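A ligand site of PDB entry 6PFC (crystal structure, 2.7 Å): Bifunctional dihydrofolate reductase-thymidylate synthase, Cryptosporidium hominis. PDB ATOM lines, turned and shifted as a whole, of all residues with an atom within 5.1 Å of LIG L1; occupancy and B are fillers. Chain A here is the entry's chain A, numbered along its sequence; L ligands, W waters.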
ATOM      1  N   VAL A   9      -2.413  32.948   7.970  1.00  0.00           N
ATOM      2  CA  VAL A   9      -2.077  31.671   8.586  1.00  0.00           C
ATOM      3  C   VAL A   9      -3.054  30.629   8.063  1.00  0.00           C
ATOM      4  O   VAL A   9      -4.274  30.835   8.146  1.00  0.00           O
ATOM      5  CB  VAL A   9      -2.111  31.743  10.116  1.00  0.00           C
ATOM      6  CG1 VAL A   9      -1.444  30.506  10.725  1.00  0.00           C
ATOM      7  CG2 VAL A   9      -1.445  33.011  10.613  1.00  0.00           C
ATOM      8  N   VAL A  10      -2.538  29.535   7.501  1.00  0.00           N
ATOM      9  CA  VAL A  10      -3.377  28.533   6.863  1.00  0.00           C
ATOM     10  C   VAL A  10      -2.645  27.201   6.882  1.00  0.00           C
ATOM     11  O   VAL A  10      -1.415  27.156   6.848  1.00  0.00           O
ATOM     12  CB  VAL A  10      -3.748  28.976   5.417  1.00  0.00           C
ATOM     13  CG1 VAL A  10      -2.494  29.148   4.568  1.00  0.00           C
ATOM     14  CG2 VAL A  10      -4.709  27.981   4.780  1.00  0.00           C
ATOM     15  N   ALA A  11      -3.419  26.121   6.942  1.00  0.00           N
ATOM     16  CA  ALA A  11      -2.921  24.755   6.789  1.00  0.00           C
ATOM     17  C   ALA A  11      -3.686  24.117   5.641  1.00  0.00           C
ATOM     18  O   ALA A  11      -4.892  23.877   5.740  1.00  0.00           O
ATOM     19  CB  ALA A  11      -3.090  23.957   8.084  1.00  0.00           C
ATOM     20  N   LEU A  25     -11.974  20.528  10.086  1.00  0.00           N
ATOM     21  CA  LEU A  25     -10.686  20.236   9.453  1.00  0.00           C
ATOM     22  C   LEU A  25     -10.644  18.784   8.983  1.00  0.00           C
ATOM     23  O   LEU A  25     -11.233  17.905   9.621  1.00  0.00           O
ATOM     24  CB  LEU A  25      -9.540  20.495  10.431  1.00  0.00           C
ATOM     25  CG  LEU A  25      -9.392  21.930  10.948  1.00  0.00           C
ATOM     26  CD1 LEU A  25      -8.328  22.000  12.031  1.00  0.00           C
ATOM     27  CD2 LEU A  25      -9.059  22.877   9.807  1.00  0.00           C
ATOM     28  N   SER A  30      -1.896  18.041  16.319  1.00  0.00           N
ATOM     29  CA  SER A  30      -1.787  18.854  17.532  1.00  0.00           C
ATOM     30  C   SER A  30      -0.718  19.924  17.389  1.00  0.00           C
ATOM     31  O   SER A  30      -0.932  21.081  17.766  1.00  0.00           O
ATOM     32  CB  SER A  30      -1.497  17.957  18.736  1.00  0.00           C
ATOM     33  OG  SER A  30      -1.269  18.723  19.897  1.00  0.00           O
ATOM     34  N   ASP A  32       0.318  21.483  14.848  1.00  0.00           N
ATOM     35  CA  ASP A  32      -0.089  22.580  13.979  1.00  0.00           C
ATOM     36  C   ASP A  32      -0.944  23.596  14.732  1.00  0.00           C
ATOM     37  O   ASP A  32      -0.815  24.807  14.511  1.00  0.00           O
ATOM     38  CB  ASP A  32      -0.841  22.047  12.769  1.00  0.00           C
ATOM     39  CG  ASP A  32      -1.412  23.146  11.899  1.00  0.00           C
ATOM     40  OD1 ASP A  32      -0.628  23.963  11.368  1.00  0.00           O
ATOM     41  OD2 ASP A  32      -2.646  23.202  11.750  1.00  0.00           O
ATOM     42  N   LEU A  33      -1.819  23.115  15.625  1.00  0.00           N
ATOM     43  CA  LEU A  33      -2.604  24.035  16.436  1.00  0.00           C
ATOM     44  C   LEU A  33      -1.713  24.821  17.390  1.00  0.00           C
ATOM     45  O   LEU A  33      -1.936  26.017  17.616  1.00  0.00           O
ATOM     46  CB  LEU A  33      -3.668  23.265  17.219  1.00  0.00           C
ATOM     47  CG  LEU A  33      -4.783  22.632  16.387  1.00  0.00           C
ATOM     48  CD1 LEU A  33      -5.812  21.964  17.285  1.00  0.00           C
ATOM     49  CD2 LEU A  33      -5.453  23.673  15.503  1.00  0.00           C
ATOM     50  N   LYS A  34      -0.687  24.174  17.948  1.00  0.00           N
ATOM     51  CA  LYS A  34       0.276  24.888  18.777  1.00  0.00           C
ATOM     52  C   LYS A  34       1.034  25.920  17.958  1.00  0.00           C
ATOM     53  O   LYS A  34       1.361  27.005  18.463  1.00  0.00           O
ATOM     54  CB  LYS A  34       1.245  23.902  19.436  1.00  0.00           C
ATOM     55  N   PHE A  35       1.317  25.612  16.699  1.00  0.00           N
ATOM     56  CA  PHE A  35       1.968  26.586  15.817  1.00  0.00           C
ATOM     57  C   PHE A  35       1.065  27.783  15.574  1.00  0.00           C
ATOM     58  O   PHE A  35       1.515  28.936  15.631  1.00  0.00           O
ATOM     59  CB  PHE A  35       2.360  25.917  14.497  1.00  0.00           C
ATOM     60  CG  PHE A  35       3.027  26.861  13.520  1.00  0.00           C
ATOM     61  CD1 PHE A  35       4.349  27.233  13.696  1.00  0.00           C
ATOM     62  CD2 PHE A  35       2.330  27.349  12.426  1.00  0.00           C
ATOM     63  CE1 PHE A  35       4.964  28.098  12.800  1.00  0.00           C
ATOM     64  CE2 PHE A  35       2.949  28.205  11.529  1.00  0.00           C
ATOM     65  CZ  PHE A  35       4.259  28.582  11.717  1.00  0.00           C
ATOM     66  N   PHE A  36      -0.225  27.538  15.301  1.00  0.00           N
ATOM     67  CA  PHE A  36      -1.174  28.636  15.137  1.00  0.00           C
ATOM     68  C   PHE A  36      -1.230  29.502  16.389  1.00  0.00           C
ATOM     69  O   PHE A  36      -1.319  30.740  16.288  1.00  0.00           O
ATOM     70  CB  PHE A  36      -2.558  28.080  14.809  1.00  0.00           C
ATOM     71  CG  PHE A  36      -3.637  29.133  14.729  1.00  0.00           C
ATOM     72  CD1 PHE A  36      -3.862  29.818  13.542  1.00  0.00           C
ATOM     73  CD2 PHE A  36      -4.413  29.437  15.830  1.00  0.00           C
ATOM     74  CE1 PHE A  36      -4.855  30.787  13.456  1.00  0.00           C
ATOM     75  CE2 PHE A  36      -5.405  30.405  15.754  1.00  0.00           C
ATOM     76  CZ  PHE A  36      -5.622  31.071  14.567  1.00  0.00           C
ATOM     77  N   SER A  37      -1.178  28.892  17.565  1.00  0.00           N
ATOM     78  CA  SER A  37      -1.241  29.659  18.808  1.00  0.00           C
ATOM     79  C   SER A  37       0.008  30.518  18.978  1.00  0.00           C
ATOM     80  O   SER A  37      -0.093  31.726  19.244  1.00  0.00           O
ATOM     81  CB  SER A  37      -1.425  28.713  19.994  1.00  0.00           C
ATOM     82  OG  SER A  37      -1.465  29.437  21.212  1.00  0.00           O
ATOM     83  N   THR A  40       0.353  33.421  16.309  1.00  0.00           N
ATOM     84  CA  THR A  40      -0.604  34.516  16.461  1.00  0.00           C
ATOM     85  C   THR A  40      -0.475  35.243  17.782  1.00  0.00           C
ATOM     86  O   THR A  40      -0.982  36.371  17.905  1.00  0.00           O
ATOM     87  CB  THR A  40      -2.046  33.990  16.306  1.00  0.00           C
ATOM     88  OG1 THR A  40      -2.257  32.912  17.232  1.00  0.00           O
ATOM     89  CG2 THR A  40      -2.285  33.495  14.884  1.00  0.00           C
ATOM     90  N   ASN A  41       0.174  34.637  18.772  1.00  0.00           N
ATOM     91  CA  ASN A  41       0.475  35.317  20.032  1.00  0.00           C
ATOM     92  C   ASN A  41       1.823  36.034  20.011  1.00  0.00           C
ATOM     93  O   ASN A  41       2.090  36.833  20.912  1.00  0.00           O
ATOM     94  CB  ASN A  41       0.462  34.308  21.187  1.00  0.00           C
ATOM     95  CG  ASN A  41      -0.940  34.039  21.716  1.00  0.00           C
ATOM     96  OD1 ASN A  41      -1.712  34.973  21.947  1.00  0.00           O
ATOM     97  ND2 ASN A  41      -1.268  32.765  21.901  1.00  0.00           N
ATOM     98  N   THR A  58     -15.874  29.845  10.035  1.00  0.00           N
ATOM     99  CA  THR A  58     -14.731  29.492  10.869  1.00  0.00           C
ATOM    100  C   THR A  58     -14.999  29.823  12.328  1.00  0.00           C
ATOM    101  O   THR A  58     -14.606  29.083  13.231  1.00  0.00           O
ATOM    102  CB  THR A  58     -13.476  30.197  10.357  1.00  0.00           C
ATOM    103  OG1 THR A  58     -13.244  29.835   8.995  1.00  0.00           O
ATOM    104  CG2 THR A  58     -12.258  29.796  11.197  1.00  0.00           C
ATOM    105  N   SER A  61     -16.866  26.984  13.650  1.00  0.00           N
ATOM    106  CA  SER A  61     -16.098  25.754  13.794  1.00  0.00           C
ATOM    107  C   SER A  61     -15.236  25.747  15.044  1.00  0.00           C
ATOM    108  O   SER A  61     -14.841  24.664  15.499  1.00  0.00           O
ATOM    109  CB  SER A  61     -15.225  25.530  12.554  1.00  0.00           C
ATOM    110  OG  SER A  61     -14.292  26.581  12.405  1.00  0.00           O
ATOM    111  N   ILE A  62     -14.902  26.917  15.599  1.00  0.00           N
ATOM    112  CA  ILE A  62     -14.109  26.993  16.821  1.00  0.00           C
ATOM    113  C   ILE A  62     -14.976  27.144  18.060  1.00  0.00           C
ATOM    114  O   ILE A  62     -14.475  27.506  19.131  1.00  0.00           O
ATOM    115  CB  ILE A  62     -13.081  28.139  16.747  1.00  0.00           C
ATOM    116  CG1 ILE A  62     -13.770  29.501  16.670  1.00  0.00           C
ATOM    117  CG2 ILE A  62     -12.149  27.955  15.557  1.00  0.00           C
ATOM    118  CD1 ILE A  62     -12.814  30.665  16.720  1.00  0.00           C
ATOM    119  N   LEU A  67     -10.253  33.453  21.835  1.00  0.00           N
ATOM    120  CA  LEU A  67      -8.908  32.914  21.973  1.00  0.00           C
ATOM    121  C   LEU A  67      -8.099  33.753  22.951  1.00  0.00           C
ATOM    122  O   LEU A  67      -8.169  34.981  22.938  1.00  0.00           O
ATOM    123  CB  LEU A  67      -8.200  32.861  20.610  1.00  0.00           C
ATOM    124  CG  LEU A  67      -8.791  31.849  19.623  1.00  0.00           C
ATOM    125  CD1 LEU A  67      -8.138  31.989  18.250  1.00  0.00           C
ATOM    126  CD2 LEU A  67      -8.622  30.429  20.146  1.00  0.00           C
ATOM    127  N   ARG A  70      -5.848  37.296  22.671  1.00  0.00           N
ATOM    128  CA  ARG A  70      -6.029  37.826  21.324  1.00  0.00           C
ATOM    129  C   ARG A  70      -7.447  38.340  21.149  1.00  0.00           C
ATOM    130  O   ARG A  70      -8.351  38.027  21.936  1.00  0.00           O
ATOM    131  CB  ARG A  70      -5.712  36.768  20.260  1.00  0.00           C
ATOM    132  CG  ARG A  70      -4.238  36.482  20.081  1.00  0.00           C
ATOM    133  CD  ARG A  70      -4.013  35.045  19.640  1.00  0.00           C
ATOM    134  NE  ARG A  70      -4.422  34.108  20.683  1.00  0.00           N
ATOM    135  CZ  ARG A  70      -4.373  32.786  20.547  1.00  0.00           C
ATOM    136  NH1 ARG A  70      -3.930  32.240  19.422  1.00  0.00           N
ATOM    137  NH2 ARG A  70      -4.763  32.009  21.557  1.00  0.00           N
ATOM    138  N   VAL A 112      -4.838  36.869   9.243  1.00  0.00           N
ATOM    139  CA  VAL A 112      -6.007  36.413   8.502  1.00  0.00           C
ATOM    140  C   VAL A 112      -6.085  34.904   8.652  1.00  0.00           C
ATOM    141  O   VAL A 112      -5.206  34.177   8.191  1.00  0.00           O
ATOM    142  CB  VAL A 112      -5.947  36.829   7.031  1.00  0.00           C
ATOM    143  CG1 VAL A 112      -7.104  36.218   6.257  1.00  0.00           C
ATOM    144  CG2 VAL A 112      -5.967  38.352   6.909  1.00  0.00           C
ATOM    145  N   CYS A 113      -7.142  34.423   9.313  1.00  0.00           N
ATOM    146  CA  CYS A 113      -7.313  33.010   9.591  1.00  0.00           C
ATOM    147  C   CYS A 113      -8.574  32.412   8.998  1.00  0.00           C
ATOM    148  O   CYS A 113      -8.745  31.185   9.064  1.00  0.00           O
ATOM    149  CB  CYS A 113      -7.323  32.770  11.115  1.00  0.00           C
ATOM    150  SG  CYS A 113      -6.224  33.850  12.053  1.00  0.00           S
ATOM    151  N   TYR A 119      -9.790  34.280   2.711  1.00  0.00           N
ATOM    152  CA  TYR A 119      -8.480  34.179   2.074  1.00  0.00           C
ATOM    153  C   TYR A 119      -8.504  34.784   0.670  1.00  0.00           C
ATOM    154  O   TYR A 119      -7.607  35.548   0.292  1.00  0.00           O
ATOM    155  CB  TYR A 119      -8.030  32.725   2.010  1.00  0.00           C
ATOM    156  CG  TYR A 119      -7.573  32.151   3.339  1.00  0.00           C
ATOM    157  CD1 TYR A 119      -6.947  32.944   4.288  1.00  0.00           C
ATOM    158  CD2 TYR A 119      -7.759  30.806   3.620  1.00  0.00           C
ATOM    159  CE1 TYR A 119      -6.531  32.417   5.492  1.00  0.00           C
ATOM    160  CE2 TYR A 119      -7.349  30.266   4.825  1.00  0.00           C
ATOM    161  CZ  TYR A 119      -6.729  31.069   5.755  1.00  0.00           C
ATOM    162  OH  TYR A 119      -6.320  30.528   6.950  1.00  0.00           O
ATOM    163  N   THR A 134       1.073  25.741   6.264  1.00  0.00           N
ATOM    164  CA  THR A 134       1.364  24.394   6.716  1.00  0.00           C
ATOM    165  C   THR A 134       0.898  23.436   5.626  1.00  0.00           C
ATOM    166  O   THR A 134      -0.305  23.295   5.400  1.00  0.00           O
ATOM    167  CB  THR A 134       0.694  24.088   8.050  1.00  0.00           C
ATOM    168  OG1 THR A 134       1.110  25.045   9.037  1.00  0.00           O
ATOM    169  CG2 THR A 134       1.051  22.690   8.520  1.00  0.00           C
HETATM  170  N1  LIG L   1      -3.811  25.706  11.010  1.00  0.00           N
HETATM  171  C1  LIG L   1      -3.009  26.639  10.466  1.00  0.00           C
HETATM  172  N2  LIG L   1      -1.652  26.277  10.135  1.00  0.00           N
HETATM  173  N3  LIG L   1      -3.431  27.889  10.231  1.00  0.00           N
HETATM  174  C2  LIG L   1      -4.699  28.255  10.525  1.00  0.00           C
HETATM  175  N4  LIG L   1      -5.182  29.578  10.290  1.00  0.00           N
HETATM  176  C3  LIG L   1      -5.574  27.303  11.102  1.00  0.00           C
HETATM  177  N5  LIG L   1      -6.865  27.627  11.421  1.00  0.00           N
HETATM  178  C4  LIG L   1      -7.654  26.689  11.962  1.00  0.00           C
HETATM  179  C5  LIG L   1      -7.200  25.386  12.202  1.00  0.00           C
HETATM  180  N6  LIG L   1      -5.926  25.077  11.886  1.00  0.00           N
HETATM  181  C6  LIG L   1      -5.098  26.021  11.328  1.00  0.00           C
HETATM  182  C7  LIG L   1      -9.085  27.053  12.315  1.00  0.00           C
HETATM  183  N7  LIG L   1      -9.630  26.337  13.444  1.00  0.00           N
HETATM  184  C8  LIG L   1     -10.770  25.468  13.255  1.00  0.00           C
HETATM  185  C9  LIG L   1      -7.911  26.749  17.317  1.00  0.00           C
HETATM  186  C10 LIG L   1      -8.515  25.562  16.921  1.00  0.00           C
HETATM  187  C11 LIG L   1      -9.078  25.437  15.658  1.00  0.00           C
HETATM  188  C12 LIG L   1      -9.039  26.500  14.772  1.00  0.00           C
HETATM  189  C13 LIG L   1      -8.429  27.692  15.147  1.00  0.00           C
HETATM  190  C14 LIG L   1      -7.865  27.816  16.419  1.00  0.00           C
HETATM  191  C15 LIG L   1      -7.302  26.862  18.693  1.00  0.00           C
HETATM  192  O1  LIG L   1      -7.809  26.230  19.612  1.00  0.00           O
HETATM  193  N8  LIG L   1      -6.139  27.681  18.969  1.00  0.00           N
HETATM  194  C16 LIG L   1      -5.598  27.750  20.296  1.00  0.00           C
HETATM  195  C17 LIG L   1      -4.964  29.071  20.474  1.00  0.00           C
HETATM  196  O2  LIG L   1      -4.952  29.894  19.521  1.00  0.00           O
HETATM  197  O3  LIG L   1      -4.437  29.386  21.591  1.00  0.00           O
HETATM  198  C18 LIG L   1      -4.524  26.733  20.428  1.00  0.00           C
HETATM  199  C19 LIG L   1      -4.870  25.348  20.880  1.00  0.00           C
HETATM  200  C20 LIG L   1      -3.722  24.490  21.294  1.00  0.00           C
HETATM  201  O4  LIG L   1      -2.750  25.034  21.857  1.00  0.00           O
HETATM  202  O5  LIG L   1      -3.542  23.387  20.720  1.00  0.00           O
HETATM  203  P1  LG2 L   2     -15.698  31.111   5.958  1.00  0.00           P
HETATM  204  O1  LG2 L   2     -14.879  31.788   4.873  1.00  0.00           O
HETATM  205  O2  LG2 L   2     -14.800  30.780   7.119  1.00  0.00           O
HETATM  206  O3  LG2 L   2     -16.781  32.069   6.456  1.00  0.00           O
HETATM  207  C1  LG2 L   2     -17.789  32.531   5.579  1.00  0.00           C
HETATM  208  C2  LG2 L   2     -18.720  33.533   6.112  1.00  0.00           C
HETATM  209  O4  LG2 L   2     -18.053  34.757   6.324  1.00  0.00           O
HETATM  210  C3  LG2 L   2     -19.799  33.843   5.175  1.00  0.00           C
HETATM  211  O5  LG2 L   2     -20.856  32.952   5.286  1.00  0.00           O
HETATM  212  C4  LG2 L   2     -20.189  35.166   5.604  1.00  0.00           C
HETATM  213  O6  LG2 L   2     -20.944  35.117   6.782  1.00  0.00           O
HETATM  214  C5  LG2 L   2     -18.916  35.799   5.901  1.00  0.00           C
HETATM  215  N1  LG2 L   2     -18.418  36.456   4.740  1.00  0.00           N
HETATM  216  C6  LG2 L   2     -17.505  35.954   3.857  1.00  0.00           C
HETATM  217  N2  LG2 L   2     -17.279  36.869   2.897  1.00  0.00           N
HETATM  218  C7  LG2 L   2     -18.048  37.974   3.158  1.00  0.00           C
HETATM  219  C8  LG2 L   2     -18.239  39.233   2.516  1.00  0.00           C
HETATM  220  N3  LG2 L   2     -17.484  39.532   1.278  1.00  0.00           N
HETATM  221  N4  LG2 L   2     -19.093  40.147   3.045  1.00  0.00           N
HETATM  222  C9  LG2 L   2     -19.766  39.843   4.188  1.00  0.00           C
HETATM  223  N5  LG2 L   2     -19.631  38.670   4.819  1.00  0.00           N
HETATM  224  C10 LG2 L   2     -18.766  37.715   4.329  1.00  0.00           C
HETATM  225  O7  LG2 L   2     -16.384  29.785   5.403  1.00  0.00           O
HETATM  226  P2  LG2 L   2     -15.536  28.610   4.752  1.00  0.00           P
HETATM  227  O8  LG2 L   2     -16.460  27.491   4.240  1.00  0.00           O
HETATM  228  O9  LG2 L   2     -14.752  29.172   3.581  1.00  0.00           O
HETATM  229  O10 LG2 L   2     -14.529  28.003   5.863  1.00  0.00           O
HETATM  230  C11 LG2 L   2     -14.899  26.866   6.613  1.00  0.00           C
HETATM  231  C12 LG2 L   2     -14.060  25.680   6.512  1.00  0.00           C
HETATM  232  O11 LG2 L   2     -12.691  26.061   6.355  1.00  0.00           O
HETATM  233  C13 LG2 L   2     -14.131  24.880   7.740  1.00  0.00           C
HETATM  234  O12 LG2 L   2     -14.050  23.530   7.416  1.00  0.00           O
HETATM  235  C14 LG2 L   2     -12.972  25.269   8.462  1.00  0.00           C
HETATM  236  O13 LG2 L   2     -12.587  24.260   9.345  1.00  0.00           O
HETATM  237  C15 LG2 L   2     -11.984  25.463   7.386  1.00  0.00           C
HETATM  238  N6  LG2 L   2     -10.879  26.281   7.825  1.00  0.00           N
HETATM  239  C16 LG2 L   2      -9.638  25.811   7.646  1.00  0.00           C
HETATM  240  C17 LG2 L   2      -8.521  26.559   8.062  1.00  0.00           C
HETATM  241  C18 LG2 L   2      -7.129  25.989   7.836  1.00  0.00           C
HETATM  242  O14 LG2 L   2      -6.137  26.689   8.111  1.00  0.00           O
HETATM  243  N7  LG2 L   2      -6.944  24.671   7.301  1.00  0.00           N
HETATM  244  C19 LG2 L   2      -8.703  27.820   8.668  1.00  0.00           C
HETATM  245  C20 LG2 L   2     -10.017  28.274   8.829  1.00  0.00           C
HETATM  246  C21 LG2 L   2     -11.091  27.499   8.415  1.00  0.00           C
HETATM  247  P3  LG2 L   2     -22.449  35.521   6.794  1.00  0.00           P
HETATM  248  O15 LG2 L   2     -23.250  34.432   6.057  1.00  0.00           O
HETATM  249  O16 LG2 L   2     -22.900  35.626   8.193  1.00  0.00           O
HETATM  250  O17 LG2 L   2     -22.658  36.848   6.145  1.00  0.00           O
HETATM  251  O   HOH W   1      -3.063  20.980  20.799  1.00  0.00           O
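Water W1 bridges O5 of LIG L1 and OG of Ser 30.
Residues that only touch LIG L1: Ala 11 (3.4 Å), Leu 25 (3.6 Å), Leu 33 (3.5 Å), Phe 36 (3.4 Å), Ser 61 (3.8 Å), Ile 62 (3.5 Å), Leu 67 (3.8 Å), Cys 113 (3.9 Å) and Tyr 119 (3.7 Å).
Of the 22 residues printed, 15 come within 4 Å of LIG L1.
The guanidinium group of Arg 70 is in salt-bridge range of an oxygen (O2) of LIG L1 (2.6 Å).
A nitrogen (N4) of LIG L1 lies within hydrogen-bond range of the backbone carbonyl oxygen of Val 9 (2.6 Å).
The side-chain carboxylate (OD1) of Asp 32 lies within hydrogen-bond range of a nitrogen (N2) of LIG L1, at 2.8 Å.
OG of Ser 37 sits at hydrogen-bond distance from O3 of LIG L1 (3.0 Å).
A nitrogen (N2) of LIG L1 is in hydrogen-bond range of the side-chain hydroxyl (OG1) of Thr 134 (3.2 Å).
A nitrogen (N3) of LIG L1 is in hydrogen-bond range of the backbone NH of Val 10.
The backbone carbonyl oxygen of Val 10 lies within hydrogen-bond range of a nitrogen (N2) of LIG L1 (3.4 Å).
O14 of LG2 L2 is in hydrogen-bond range of N of Ala 11 (3.0 Å).
The backbone carbonyl oxygen (O) of Ala 11 is in hydrogen-bond range of a nitrogen (N7) of LG2 L2.
The backbone NH of Thr 58 lies within hydrogen-bond range of an oxygen (O2) of LG2 L2.
The side-chain hydroxyl of Thr 58 is in hydrogen-bond range of an oxygen (O2) of LG2 L2, 2.6 Å away.
The side-chain amide oxygen of Asn 41 is in hydrogen-bond range of the guanidinium group of Arg 70 (3.1 Å).
The guanidinium group (NH1) of Arg 70 sits at hydrogen-bond distance from the side-chain hydroxyl (OG1) of Thr 40 (2.8 Å).
The backbone carbonyl oxygen of Val 112 is in hydrogen-bond range of the backbone NH of Val 9, at 3.1 Å.
The backbone carbonyl oxygen of Ser 37 sits at hydrogen-bond distance from the side-chain amide nitrogen of Asn 41, 3.1 Å away.
The backbone carbonyl oxygen (O) of Val 10 lies within hydrogen-bond range of the backbone NH (N) of Thr 134, at 2.9 Å.
The backbone carbonyl oxygen of Phe 36 is in hydrogen-bond range of the side-chain hydroxyl of Thr 40 (2.5 Å).
O of Cys 113 lies within hydrogen-bond range of OH of Tyr 119 (3.3 Å).
The backbone carbonyl oxygen (O) of Thr 58 is in hydrogen-bond range of the side-chain hydroxyl (OG) of Ser 61, 2.7 Å away.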
